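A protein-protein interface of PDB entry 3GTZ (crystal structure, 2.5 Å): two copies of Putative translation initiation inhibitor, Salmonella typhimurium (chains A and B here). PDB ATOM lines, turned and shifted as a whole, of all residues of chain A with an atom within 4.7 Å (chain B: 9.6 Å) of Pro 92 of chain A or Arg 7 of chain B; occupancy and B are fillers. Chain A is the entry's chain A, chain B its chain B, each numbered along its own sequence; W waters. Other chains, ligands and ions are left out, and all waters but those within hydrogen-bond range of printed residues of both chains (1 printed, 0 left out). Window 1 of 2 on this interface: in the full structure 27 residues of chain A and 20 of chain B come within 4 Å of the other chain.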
ATOM      1  N   SER A  60      22.733  12.628 -29.290  1.00  0.00           N
ATOM      2  CA  SER A  60      22.175  13.744 -28.547  1.00  0.00           C
ATOM      3  C   SER A  60      21.443  14.650 -29.468  1.00  0.00           C
ATOM      4  O   SER A  60      20.810  15.551 -28.967  1.00  0.00           O
ATOM      5  CB  SER A  60      23.245  14.645 -27.886  1.00  0.00           C
ATOM      6  OG  SER A  60      24.477  14.010 -27.800  1.00  0.00           O
ATOM      7  N   ARG A  61      21.608  14.479 -30.787  1.00  0.00           N
ATOM      8  CA  ARG A  61      21.063  15.413 -31.759  1.00  0.00           C
ATOM      9  C   ARG A  61      19.872  14.835 -32.504  1.00  0.00           C
ATOM     10  O   ARG A  61      19.452  15.382 -33.502  1.00  0.00           O
ATOM     11  CB  ARG A  61      22.129  15.850 -32.750  1.00  0.00           C
ATOM     12  CG  ARG A  61      23.438  16.445 -32.113  1.00  0.00           C
ATOM     13  CD  ARG A  61      23.495  17.956 -32.128  1.00  0.00           C
ATOM     14  NE  ARG A  61      23.532  18.465 -33.495  1.00  0.00           N
ATOM     15  CZ  ARG A  61      23.123  19.677 -33.881  1.00  0.00           C
ATOM     16  NH1 ARG A  61      22.639  20.538 -33.007  1.00  0.00           N
ATOM     17  NH2 ARG A  61      23.193  20.026 -35.157  1.00  0.00           N
ATOM     18  N   ILE A  62      19.303  13.745 -32.010  1.00  0.00           N
ATOM     19  CA  ILE A  62      18.194  13.123 -32.694  1.00  0.00           C
ATOM     20  C   ILE A  62      16.958  13.896 -32.288  1.00  0.00           C
ATOM     21  O   ILE A  62      16.786  14.219 -31.119  1.00  0.00           O
ATOM     22  CB  ILE A  62      18.024  11.656 -32.307  1.00  0.00           C
ATOM     23  CG1 ILE A  62      19.218  10.828 -32.771  1.00  0.00           C
ATOM     24  CG2 ILE A  62      16.716  11.091 -32.863  1.00  0.00           C
ATOM     25  CD1 ILE A  62      19.275   9.438 -32.149  1.00  0.00           C
ATOM     26  N   LEU A  63      16.079  14.156 -33.249  1.00  0.00           N
ATOM     27  CA  LEU A  63      14.911  14.991 -33.025  1.00  0.00           C
ATOM     28  C   LEU A  63      13.662  14.176 -32.756  1.00  0.00           C
ATOM     29  O   LEU A  63      12.946  14.450 -31.811  1.00  0.00           O
ATOM     30  CB  LEU A  63      14.694  15.894 -34.226  1.00  0.00           C
ATOM     31  CG  LEU A  63      15.890  16.749 -34.624  1.00  0.00           C
ATOM     32  CD1 LEU A  63      15.637  17.377 -35.993  1.00  0.00           C
ATOM     33  CD2 LEU A  63      16.090  17.802 -33.567  1.00  0.00           C
ATOM     34  N   ASP A  64      13.421  13.163 -33.571  1.00  0.00           N
ATOM     35  CA  ASP A  64      12.217  12.345 -33.470  1.00  0.00           C
ATOM     36  C   ASP A  64      12.510  10.898 -33.831  1.00  0.00           C
ATOM     37  O   ASP A  64      13.244  10.661 -34.749  1.00  0.00           O
ATOM     38  CB  ASP A  64      11.165  12.888 -34.413  1.00  0.00           C
ATOM     39  CG  ASP A  64       9.841  12.185 -34.256  1.00  0.00           C
ATOM     40  OD1 ASP A  64       9.137  12.407 -33.258  1.00  0.00           O
ATOM     41  OD2 ASP A  64       9.513  11.375 -35.116  1.00  0.00           O
ATOM     42  N   ALA A  65      11.940   9.940 -33.112  1.00  0.00           N
ATOM     43  CA  ALA A  65      12.165   8.508 -33.389  1.00  0.00           C
ATOM     44  C   ALA A  65      10.846   7.747 -33.366  1.00  0.00           C
ATOM     45  O   ALA A  65      10.032   7.922 -32.481  1.00  0.00           O
ATOM     46  CB  ALA A  65      13.140   7.889 -32.377  1.00  0.00           C
ATOM     47  N   TRP A  82      16.470   0.652 -25.401  1.00  0.00           N
ATOM     48  CA  TRP A  82      16.381   2.108 -25.487  1.00  0.00           C
ATOM     49  C   TRP A  82      16.908   2.741 -24.215  1.00  0.00           C
ATOM     50  O   TRP A  82      17.683   3.694 -24.278  1.00  0.00           O
ATOM     51  CB  TRP A  82      14.932   2.529 -25.707  1.00  0.00           C
ATOM     52  CG  TRP A  82      14.709   3.988 -25.750  1.00  0.00           C
ATOM     53  CD1 TRP A  82      14.478   4.797 -24.692  1.00  0.00           C
ATOM     54  CD2 TRP A  82      14.662   4.825 -26.911  1.00  0.00           C
ATOM     55  NE1 TRP A  82      14.311   6.083 -25.103  1.00  0.00           N
ATOM     56  CE2 TRP A  82      14.389   6.129 -26.465  1.00  0.00           C
ATOM     57  CE3 TRP A  82      14.809   4.593 -28.281  1.00  0.00           C
ATOM     58  CZ2 TRP A  82      14.278   7.202 -27.323  1.00  0.00           C
ATOM     59  CZ3 TRP A  82      14.682   5.659 -29.146  1.00  0.00           C
ATOM     60  CH2 TRP A  82      14.440   6.957 -28.665  1.00  0.00           C
ATOM     61  N   GLY A  89      18.109  13.758 -20.621  1.00  0.00           N
ATOM     62  CA  GLY A  89      18.021  15.198 -20.918  1.00  0.00           C
ATOM     63  C   GLY A  89      18.188  15.593 -22.390  1.00  0.00           C
ATOM     64  O   GLY A  89      17.990  16.756 -22.731  1.00  0.00           O
ATOM     65  N   HIS A  90      18.557  14.646 -23.259  1.00  0.00           N
ATOM     66  CA  HIS A  90      18.808  14.947 -24.668  1.00  0.00           C
ATOM     67  C   HIS A  90      18.078  13.942 -25.583  1.00  0.00           C
ATOM     68  O   HIS A  90      18.485  13.685 -26.697  1.00  0.00           O
ATOM     69  CB  HIS A  90      20.312  14.955 -24.928  1.00  0.00           C
ATOM     70  CG  HIS A  90      21.028  16.044 -24.209  1.00  0.00           C
ATOM     71  ND1 HIS A  90      21.188  17.306 -24.741  1.00  0.00           N
ATOM     72  CD2 HIS A  90      21.577  16.085 -22.970  1.00  0.00           C
ATOM     73  CE1 HIS A  90      21.828  18.067 -23.874  1.00  0.00           C
ATOM     74  NE2 HIS A  90      22.084  17.349 -22.794  1.00  0.00           N
ATOM     75  N   ALA A  91      16.988  13.395 -25.082  1.00  0.00           N
ATOM     76  CA  ALA A  91      16.221  12.386 -25.782  1.00  0.00           C
ATOM     77  C   ALA A  91      15.266  13.020 -26.838  1.00  0.00           C
ATOM     78  O   ALA A  91      14.703  14.094 -26.630  1.00  0.00           O
ATOM     79  CB  ALA A  91      15.408  11.590 -24.762  1.00  0.00           C
ATOM     80  N   PRO A  92      15.019  12.321 -27.940  1.00  0.00           N
ATOM     81  CA  PRO A  92      14.064  12.845 -28.900  1.00  0.00           C
ATOM     82  C   PRO A  92      12.610  12.568 -28.502  1.00  0.00           C
ATOM     83  O   PRO A  92      12.355  11.860 -27.518  1.00  0.00           O
ATOM     84  CB  PRO A  92      14.413  12.081 -30.151  1.00  0.00           C
ATOM     85  CG  PRO A  92      14.865  10.751 -29.632  1.00  0.00           C
ATOM     86  CD  PRO A  92      15.546  11.009 -28.329  1.00  0.00           C
ATOM     87  N   VAL A  93      11.667  13.139 -29.249  1.00  0.00           N
ATOM     88  CA  VAL A  93      10.276  12.673 -29.222  1.00  0.00           C
ATOM     89  C   VAL A  93      10.284  11.227 -29.667  1.00  0.00           C
ATOM     90  O   VAL A  93      11.020  10.843 -30.553  1.00  0.00           O
ATOM     91  CB  VAL A  93       9.335  13.508 -30.136  1.00  0.00           C
ATOM     92  CG1 VAL A  93       7.906  12.963 -30.100  1.00  0.00           C
ATOM     93  CG2 VAL A  93       9.317  14.940 -29.691  1.00  0.00           C
ATOM     94  N   ARG A  94       9.510  10.404 -28.993  1.00  0.00           N
ATOM     95  CA  ARG A  94       9.528   8.981 -29.243  1.00  0.00           C
ATOM     96  C   ARG A  94       8.124   8.492 -29.395  1.00  0.00           C
ATOM     97  O   ARG A  94       7.191   8.999 -28.781  1.00  0.00           O
ATOM     98  CB  ARG A  94      10.215   8.212 -28.105  1.00  0.00           C
ATOM     99  CG  ARG A  94      10.030   6.696 -28.219  1.00  0.00           C
ATOM    100  CD  ARG A  94      11.179   5.944 -27.693  1.00  0.00           C
ATOM    101  NE  ARG A  94      11.018   5.585 -26.301  1.00  0.00           N
ATOM    102  CZ  ARG A  94      10.538   4.427 -25.869  1.00  0.00           C
ATOM    103  NH1 ARG A  94      10.132   3.503 -26.714  1.00  0.00           N
ATOM    104  NH2 ARG A  94      10.436   4.208 -24.561  1.00  0.00           N
ATOM    105  N   SER B   4      20.038  25.527 -33.157  1.00  0.00           N
ATOM    106  CA  SER B   4      20.187  24.972 -31.812  1.00  0.00           C
ATOM    107  C   SER B   4      18.900  24.194 -31.530  1.00  0.00           C
ATOM    108  O   SER B   4      17.829  24.613 -31.963  1.00  0.00           O
ATOM    109  CB  SER B   4      20.434  26.083 -30.756  1.00  0.00           C
ATOM    110  N   ILE B   5      19.026  23.052 -30.847  1.00  0.00           N
ATOM    111  CA  ILE B   5      17.906  22.186 -30.526  1.00  0.00           C
ATOM    112  C   ILE B   5      17.377  22.592 -29.181  1.00  0.00           C
ATOM    113  O   ILE B   5      18.128  22.628 -28.212  1.00  0.00           O
ATOM    114  CB  ILE B   5      18.328  20.690 -30.408  1.00  0.00           C
ATOM    115  CG1 ILE B   5      18.826  20.136 -31.743  1.00  0.00           C
ATOM    116  CG2 ILE B   5      17.160  19.822 -29.977  1.00  0.00           C
ATOM    117  CD1 ILE B   5      19.257  18.668 -31.676  1.00  0.00           C
ATOM    118  N   VAL B   6      16.081  22.866 -29.106  1.00  0.00           N
ATOM    119  CA  VAL B   6      15.410  23.124 -27.850  1.00  0.00           C
ATOM    120  C   VAL B   6      14.470  21.969 -27.534  1.00  0.00           C
ATOM    121  O   VAL B   6      13.675  21.581 -28.364  1.00  0.00           O
ATOM    122  CB  VAL B   6      14.650  24.462 -27.940  1.00  0.00           C
ATOM    123  CG1 VAL B   6      13.746  24.690 -26.711  1.00  0.00           C
ATOM    124  CG2 VAL B   6      15.669  25.600 -28.146  1.00  0.00           C
ATOM    125  N   ARG B   7      14.573  21.421 -26.327  1.00  0.00           N
ATOM    126  CA  ARG B   7      13.704  20.339 -25.854  1.00  0.00           C
ATOM    127  C   ARG B   7      12.816  20.795 -24.673  1.00  0.00           C
ATOM    128  O   ARG B   7      13.325  21.389 -23.732  1.00  0.00           O
ATOM    129  CB  ARG B   7      14.567  19.141 -25.448  1.00  0.00           C
ATOM    130  CG  ARG B   7      15.548  18.684 -26.565  1.00  0.00           C
ATOM    131  CD  ARG B   7      16.305  17.406 -26.246  1.00  0.00           C
ATOM    132  NE  ARG B   7      17.358  17.140 -27.243  1.00  0.00           N
ATOM    133  CZ  ARG B   7      17.237  16.308 -28.280  1.00  0.00           C
ATOM    134  NH1 ARG B   7      16.124  15.620 -28.473  1.00  0.00           N
ATOM    135  NH2 ARG B   7      18.235  16.159 -29.136  1.00  0.00           N
ATOM    136  N   ILE B   8      11.505  20.518 -24.742  1.00  0.00           N
ATOM    137  CA  ILE B   8      10.561  20.812 -23.682  1.00  0.00           C
ATOM    138  C   ILE B   8      10.204  19.545 -22.936  1.00  0.00           C
ATOM    139  O   ILE B   8       9.917  18.510 -23.552  1.00  0.00           O
ATOM    140  CB  ILE B   8       9.241  21.418 -24.228  1.00  0.00           C
ATOM    141  CG1 ILE B   8       9.525  22.578 -25.186  1.00  0.00           C
ATOM    142  CG2 ILE B   8       8.327  21.928 -23.097  1.00  0.00           C
ATOM    143  CD1 ILE B   8      10.396  23.642 -24.555  1.00  0.00           C
ATOM    144  N   ASP B   9      10.189  19.651 -21.597  1.00  0.00           N
ATOM    145  CA  ASP B   9      10.014  18.514 -20.670  1.00  0.00           C
ATOM    146  C   ASP B   9      10.953  17.366 -21.036  1.00  0.00           C
ATOM    147  O   ASP B   9      10.551  16.280 -21.402  1.00  0.00           O
ATOM    148  CB  ASP B   9       8.532  18.086 -20.510  1.00  0.00           C
ATOM    149  N   ALA B  10      12.230  17.659 -20.901  1.00  0.00           N
ATOM    150  CA  ALA B  10      13.310  16.761 -21.229  1.00  0.00           C
ATOM    151  C   ALA B  10      13.628  15.815 -20.055  1.00  0.00           C
ATOM    152  O   ALA B  10      14.313  16.178 -19.120  1.00  0.00           O
ATOM    153  CB  ALA B  10      14.557  17.588 -21.609  1.00  0.00           C
ATOM    154  N   GLU B  11      13.154  14.591 -20.132  1.00  0.00           N
ATOM    155  CA  GLU B  11      13.343  13.649 -19.054  1.00  0.00           C
ATOM    156  C   GLU B  11      14.529  12.706 -19.357  1.00  0.00           C
ATOM    157  O   GLU B  11      15.357  13.004 -20.231  1.00  0.00           O
ATOM    158  CB  GLU B  11      12.024  12.906 -18.799  1.00  0.00           C
ATOM    159  CG  GLU B  11      10.836  13.837 -18.426  1.00  0.00           C
ATOM    160  CD  GLU B  11      10.969  14.553 -17.049  1.00  0.00           C
ATOM    161  OE1 GLU B  11      10.284  14.134 -16.081  1.00  0.00           O
ATOM    162  OE2 GLU B  11      11.728  15.540 -16.927  1.00  0.00           O
ATOM    163  N   ASP B  12      14.632  11.612 -18.606  1.00  0.00           N
ATOM    164  CA  ASP B  12      15.738  10.664 -18.713  1.00  0.00           C
ATOM    165  C   ASP B  12      15.621   9.781 -19.958  1.00  0.00           C
ATOM    166  O   ASP B  12      16.628   9.399 -20.542  1.00  0.00           O
ATOM    167  CB  ASP B  12      15.775   9.749 -17.467  1.00  0.00           C
ATOM    168  CG  ASP B  12      16.311  10.460 -16.206  1.00  0.00           C
ATOM    169  OD1 ASP B  12      17.110  11.436 -16.306  1.00  0.00           O
ATOM    170  OD2 ASP B  12      15.927  10.014 -15.102  1.00  0.00           O
ATOM    171  N   ARG B  13      14.393   9.438 -20.333  1.00  0.00           N
ATOM    172  CA  ARG B  13      14.134   8.495 -21.417  1.00  0.00           C
ATOM    173  C   ARG B  13      13.372   9.067 -22.604  1.00  0.00           C
ATOM    174  O   ARG B  13      13.324   8.440 -23.643  1.00  0.00           O
ATOM    175  CB  ARG B  13      13.424   7.254 -20.872  1.00  0.00           C
ATOM    176  CG  ARG B  13      14.321   6.480 -19.897  1.00  0.00           C
ATOM    177  CD  ARG B  13      13.583   5.556 -18.957  1.00  0.00           C
ATOM    178  NE  ARG B  13      14.542   4.871 -18.088  1.00  0.00           N
ATOM    179  CZ  ARG B  13      14.260   3.898 -17.212  1.00  0.00           C
ATOM    180  NH1 ARG B  13      13.024   3.445 -17.048  1.00  0.00           N
ATOM    181  NH2 ARG B  13      15.244   3.367 -16.499  1.00  0.00           N
ATOM    182  N   TRP B  14      12.808  10.265 -22.465  1.00  0.00           N
ATOM    183  CA  TRP B  14      12.088  10.909 -23.561  1.00  0.00           C
ATOM    184  C   TRP B  14      12.027  12.402 -23.353  1.00  0.00           C
ATOM    185  O   TRP B  14      12.317  12.868 -22.263  1.00  0.00           O
ATOM    186  CB  TRP B  14      10.661  10.329 -23.692  1.00  0.00           C
ATOM    187  CG  TRP B  14      10.048  10.012 -22.386  1.00  0.00           C
ATOM    188  CD1 TRP B  14      10.013   8.782 -21.755  1.00  0.00           C
ATOM    189  CD2 TRP B  14       9.420  10.933 -21.505  1.00  0.00           C
ATOM    190  NE1 TRP B  14       9.384   8.891 -20.527  1.00  0.00           N
ATOM    191  CE2 TRP B  14       9.003  10.200 -20.352  1.00  0.00           C
ATOM    192  CE3 TRP B  14       9.140  12.297 -21.579  1.00  0.00           C
ATOM    193  CZ2 TRP B  14       8.325  10.804 -19.284  1.00  0.00           C
ATOM    194  CZ3 TRP B  14       8.470  12.902 -20.529  1.00  0.00           C
ATOM    195  CH2 TRP B  14       8.071  12.157 -19.386  1.00  0.00           C
ATOM    196  N   SER B  15      11.691  13.131 -24.428  1.00  0.00           N
ATOM    197  CA  SER B  15      11.273  14.536 -24.382  1.00  0.00           C
ATOM    198  C   SER B  15       9.819  14.648 -24.884  1.00  0.00           C
ATOM    199  O   SER B  15       9.387  13.876 -25.754  1.00  0.00           O
ATOM    200  CB  SER B  15      12.158  15.399 -25.263  1.00  0.00           C
ATOM    201  OG  SER B  15      13.445  15.601 -24.713  1.00  0.00           O
ATOM    202  N   ASP B  16       9.064  15.607 -24.363  1.00  0.00           N
ATOM    203  CA  ASP B  16       7.665  15.771 -24.801  1.00  0.00           C
ATOM    204  C   ASP B  16       7.541  16.575 -26.123  1.00  0.00           C
ATOM    205  O   ASP B  16       6.739  16.201 -26.983  1.00  0.00           O
ATOM    206  CB  ASP B  16       6.851  16.449 -23.701  1.00  0.00           C
ATOM    207  CG  ASP B  16       5.361  16.332 -23.915  1.00  0.00           C
ATOM    208  OD1 ASP B  16       4.879  15.191 -24.178  1.00  0.00           O
ATOM    209  OD2 ASP B  16       4.678  17.393 -23.773  1.00  0.00           O
ATOM    210  N   VAL B  17       8.332  17.645 -26.256  1.00  0.00           N
ATOM    211  CA  VAL B  17       8.381  18.489 -27.440  1.00  0.00           C
ATOM    212  C   VAL B  17       9.826  18.816 -27.812  1.00  0.00           C
ATOM    213  O   VAL B  17      10.666  18.985 -26.921  1.00  0.00           O
ATOM    214  CB  VAL B  17       7.709  19.812 -27.189  1.00  0.00           C
ATOM    215  CG1 VAL B  17       7.541  20.575 -28.492  1.00  0.00           C
ATOM    216  CG2 VAL B  17       6.374  19.579 -26.429  1.00  0.00           C
ATOM    217  N   VAL B  18      10.118  18.872 -29.117  1.00  0.00           N
ATOM    218  CA  VAL B  18      11.456  19.187 -29.623  1.00  0.00           C
ATOM    219  C   VAL B  18      11.364  20.207 -30.756  1.00  0.00           C
ATOM    220  O   VAL B  18      10.538  20.060 -31.645  1.00  0.00           O
ATOM    221  CB  VAL B  18      12.145  17.924 -30.150  1.00  0.00           C
ATOM    222  CG1 VAL B  18      13.362  18.275 -30.915  1.00  0.00           C
ATOM    223  CG2 VAL B  18      12.516  16.996 -29.032  1.00  0.00           C
ATOM    224  N   ILE B  19      12.202  21.233 -30.721  1.00  0.00           N
ATOM    225  CA  ILE B  19      12.108  22.356 -31.624  1.00  0.00           C
ATOM    226  C   ILE B  19      13.478  22.602 -32.204  1.00  0.00           C
ATOM    227  O   ILE B  19      14.450  22.725 -31.489  1.00  0.00           O
ATOM    228  CB  ILE B  19      11.618  23.620 -30.919  1.00  0.00           C
ATOM    229  CG1 ILE B  19      10.252  23.362 -30.251  1.00  0.00           C
ATOM    230  CG2 ILE B  19      11.544  24.823 -31.899  1.00  0.00           C
ATOM    231  CD1 ILE B  19       9.818  24.509 -29.453  1.00  0.00           C
ATOM    232  N   TYR B  20      13.544  22.658 -33.524  1.00  0.00           N
ATOM    233  CA  TYR B  20      14.793  22.799 -34.228  1.00  0.00           C
ATOM    234  C   TYR B  20      14.460  23.309 -35.635  1.00  0.00           C
ATOM    235  O   TYR B  20      13.477  22.864 -36.257  1.00  0.00           O
ATOM    236  CB  TYR B  20      15.474  21.433 -34.303  1.00  0.00           C
ATOM    237  CG  TYR B  20      16.671  21.375 -35.237  1.00  0.00           C
ATOM    238  CD1 TYR B  20      17.877  21.963 -34.897  1.00  0.00           C
ATOM    239  CD2 TYR B  20      16.593  20.728 -36.454  1.00  0.00           C
ATOM    240  CE1 TYR B  20      18.955  21.909 -35.742  1.00  0.00           C
ATOM    241  CE2 TYR B  20      17.676  20.681 -37.310  1.00  0.00           C
ATOM    242  CZ  TYR B  20      18.856  21.252 -36.935  1.00  0.00           C
ATOM    243  OH  TYR B  20      19.928  21.212 -37.774  1.00  0.00           O
ATOM    244  N   THR B  23      10.950  24.245 -36.618  1.00  0.00           N
ATOM    245  CA  THR B  23      10.045  23.131 -36.761  1.00  0.00           C
ATOM    246  C   THR B  23       9.939  22.419 -35.414  1.00  0.00           C
ATOM    247  O   THR B  23      10.929  22.284 -34.690  1.00  0.00           O
ATOM    248  CB  THR B  23      10.586  22.146 -37.825  1.00  0.00           C
ATOM    249  OG1 THR B  23      10.998  22.887 -38.981  1.00  0.00           O
ATOM    250  CG2 THR B  23       9.537  21.096 -38.197  1.00  0.00           C
ATOM    251  N   LEU B  24       8.735  21.943 -35.114  1.00  0.00           N
ATOM    252  CA  LEU B  24       8.389  21.366 -33.841  1.00  0.00           C
ATOM    253  C   LEU B  24       7.883  19.955 -34.057  1.00  0.00           C
ATOM    254  O   LEU B  24       7.051  19.744 -34.919  1.00  0.00           O
ATOM    255  CB  LEU B  24       7.279  22.208 -33.225  1.00  0.00           C
ATOM    256  CG  LEU B  24       6.643  21.810 -31.887  1.00  0.00           C
ATOM    257  CD1 LEU B  24       6.237  23.058 -31.131  1.00  0.00           C
ATOM    258  CD2 LEU B  24       5.443  20.836 -32.016  1.00  0.00           C
ATOM    259  N   TRP B  25       8.368  19.003 -33.254  1.00  0.00           N
ATOM    260  CA  TRP B  25       7.885  17.608 -33.229  1.00  0.00           C
ATOM    261  C   TRP B  25       7.162  17.331 -31.911  1.00  0.00           C
ATOM    262  O   TRP B  25       7.572  17.840 -30.874  1.00  0.00           O
ATOM    263  CB  TRP B  25       9.081  16.654 -33.341  1.00  0.00           C
ATOM    264  CG  TRP B  25       9.659  16.587 -34.722  1.00  0.00           C
ATOM    265  CD1 TRP B  25       9.327  15.673 -35.685  1.00  0.00           C
ATOM    266  CD2 TRP B  25      10.631  17.453 -35.312  1.00  0.00           C
ATOM    267  NE1 TRP B  25      10.037  15.916 -36.833  1.00  0.00           N
ATOM    268  CE2 TRP B  25      10.839  17.006 -36.639  1.00  0.00           C
ATOM    269  CE3 TRP B  25      11.341  18.551 -34.859  1.00  0.00           C
ATOM    270  CZ2 TRP B  25      11.723  17.623 -37.517  1.00  0.00           C
ATOM    271  CZ3 TRP B  25      12.237  19.184 -35.737  1.00  0.00           C
ATOM    272  CH2 TRP B  25      12.410  18.710 -37.058  1.00  0.00           C
ATOM    273  N   TYR B  26       6.127  16.497 -31.946  1.00  0.00           N
ATOM    274  CA  TYR B  26       5.375  16.113 -30.761  1.00  0.00           C
ATOM    275  C   TYR B  26       4.514  14.908 -31.069  1.00  0.00           C
ATOM    276  O   TYR B  26       3.932  14.867 -32.126  1.00  0.00           O
ATOM    277  CB  TYR B  26       4.472  17.279 -30.344  1.00  0.00           C
ATOM    278  CG  TYR B  26       3.499  17.003 -29.216  1.00  0.00           C
ATOM    279  CD1 TYR B  26       3.940  16.949 -27.895  1.00  0.00           C
ATOM    280  CD2 TYR B  26       2.141  16.857 -29.454  1.00  0.00           C
ATOM    281  CE1 TYR B  26       3.059  16.711 -26.826  1.00  0.00           C
ATOM    282  CE2 TYR B  26       1.243  16.615 -28.400  1.00  0.00           C
ATOM    283  CZ  TYR B  26       1.715  16.544 -27.084  1.00  0.00           C
ATOM    284  OH  TYR B  26       0.864  16.307 -26.022  1.00  0.00           O
ATOM    285  N   THR B  27       4.435  13.941 -30.157  1.00  0.00           N
ATOM    286  CA  THR B  27       3.368  12.934 -30.157  1.00  0.00           C
ATOM    287  C   THR B  27       2.320  13.215 -29.076  1.00  0.00           C
ATOM    288  O   THR B  27       2.665  13.394 -27.936  1.00  0.00           O
ATOM    289  CB  THR B  27       3.876  11.546 -29.821  1.00  0.00           C
ATOM    290  OG1 THR B  27       5.027  11.251 -30.598  1.00  0.00           O
ATOM    291  CG2 THR B  27       2.778  10.493 -30.107  1.00  0.00           C
ATOM    292  N   GLN B  55       4.490  27.410 -27.322  1.00  0.00           N
ATOM    293  CA  GLN B  55       5.718  27.719 -28.064  1.00  0.00           C
ATOM    294  C   GLN B  55       5.563  28.817 -29.109  1.00  0.00           C
ATOM    295  O   GLN B  55       6.535  29.170 -29.799  1.00  0.00           O
ATOM    296  CB  GLN B  55       6.248  26.468 -28.736  1.00  0.00           C
ATOM    297  CG  GLN B  55       6.339  25.244 -27.802  1.00  0.00           C
ATOM    298  CD  GLN B  55       7.162  25.501 -26.551  1.00  0.00           C
ATOM    299  OE1 GLN B  55       8.161  26.218 -26.587  1.00  0.00           O
ATOM    300  NE2 GLN B  55       6.757  24.893 -25.447  1.00  0.00           N
HETATM  301  O   HOH W   1      21.946  21.765 -30.542  1.00  0.00           O
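N of Asp 16 of chain B sits at hydrogen-bond distance from O of Asp 9 of chain B, at 3.4 Å.
N of Asp 16 of chain B lies within hydrogen-bond range of O of Ile 8 of chain B (3.1 Å).
The backbone carbonyl oxygen of Leu 63 of chain A is in hydrogen-bond range of the backbone NH of Val 93 of chain A (3.1 Å).
The backbone carbonyl oxygen of Val 93 of chain A lies within hydrogen-bond range of the backbone NH of Ala 65 of chain A (2.9 Å).
Of the printed residues of chain B, Pro 92 of chain A touches Arg 7 (3.5 Å) and Ser 15 (3.4 Å).
Arg 7 of chain B touches just these residues of chain A: Ser 60 (2.7 Å), Arg 61 (3.9 Å), Ile 62 (3.1 Å), Gly 89 (3.95 Å), His 90 (3.3 Å), Ala 91 (2.8 Å) and Pro 92 (3.5 Å).
Ile 62 of chain A touches just one residue of chain B: Arg 7.
Ala 91 of chain A touches just these residues of chain B: Arg 7 (2.8 Å), Arg 13 (3.9 Å), Trp 14 (3.6 Å) and Ser 15 (2.7 Å).
Printed residues of chain B within 4 Å of Leu 63 of chain A: Ile 5 (3.8 Å), Val 18 (3.8 Å), Tyr 20 (3.5 Å) and Trp 25 (3.7 Å).
Of the printed residues of chain A, Ala 10 of chain B touches Gly 89.
Ser 4 of chain B touches none of the printed residues of chain A.
The nearest residue of chain B that does not touch Pro 92 of chain A is Trp 14 of chain B (4.1 Å).
The nearest printed residue of chain A that does not touch Arg 7 of chain B is Leu 63 of chain A (4.8 Å).
Of the 13 printed residues of chain A, 12 touch a printed residue of chain B.
Hydrophobic or aromatic side chains of chain A within 4 Å of the printed part of chain B: Leu 63, Trp 82, Ala 91 and Val 93.
Of the 23 printed residues of chain B, 12 touch a printed residue of chain A.
Hydrophobic or aromatic side chains of chain B within 4 Å of the printed part of chain A: Ile 5, Ala 10, Val 18, Tyr 20 and Trp 25.
Among the printed residues, 26 pairs touch across the chains.
Among the printed residues, no Asp or Glu carboxylate lies within 4 Å of a Lys or Arg side-chain nitrogen of the other chain.
No position is printed for both chains.
Of the 26 pairs that touch across the chains among the printed residues, none has its exchanged pair printed and touching as well.
Water W1 lies within hydrogen-bond range of the guanidinium group (NH1) of Arg 61 of chain A (2.8 Å) and the backbone NH (N) of Ile 5 of chain B (3.2 Å).
The backbone NH of Gly 89 of chain A lies within hydrogen-bond range of the backbone carbonyl oxygen of Glu 11 of chain B, at 2.9 Å.
The backbone carbonyl oxygen of Pro 92 of chain A is in hydrogen-bond range of the backbone NH of Ser 15 of chain B, at 3.4 Å.
O of Ala 91 of chain A lies within hydrogen-bond range of OG of Ser 15 of chain B (2.7 Å).
NE1 of Trp 82 of chain A lies within hydrogen-bond range of O of Arg 13 of chain B (2.9 Å).
NH1 of Arg 7 of chain B lies within hydrogen-bond range of O of Ala 91 of chain A (2.8 Å).
The backbone carbonyl oxygen (O) of Ser 60 of chain A is in hydrogen-bond range of the guanidinium group (NH2) of Arg 7 of chain B.
The backbone carbonyl oxygen of Ile 62 of chain A sits at hydrogen-bond distance from the guanidinium group of Arg 7 of chain B (3.1 Å).
O of His 90 of chain A sits close to NH2 of Arg 7 of chain B (3.5 Å).
Arg 7 of chain B touches Arg 61 of chain A (NH2 to CA, 3.9 Å).
CD1 of Leu 63 of chain A touches CD2 of Tyr 20 of chain B, at 3.5 Å.
CB of Asp 64 of chain A touches CD1 of Trp 25 of chain B, at 3.6 Å.
C of Arg 13 of chain B touches CB of Ala 91 of chain A, at 3.9 Å.
Trp 14 of chain B touches Ala 91 of chain A (CA to CB, 3.6 Å).
Arg 7 of chain B touches Pro 92 of chain A.
Asp 16 of chain B touches Val 93 of chain A.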
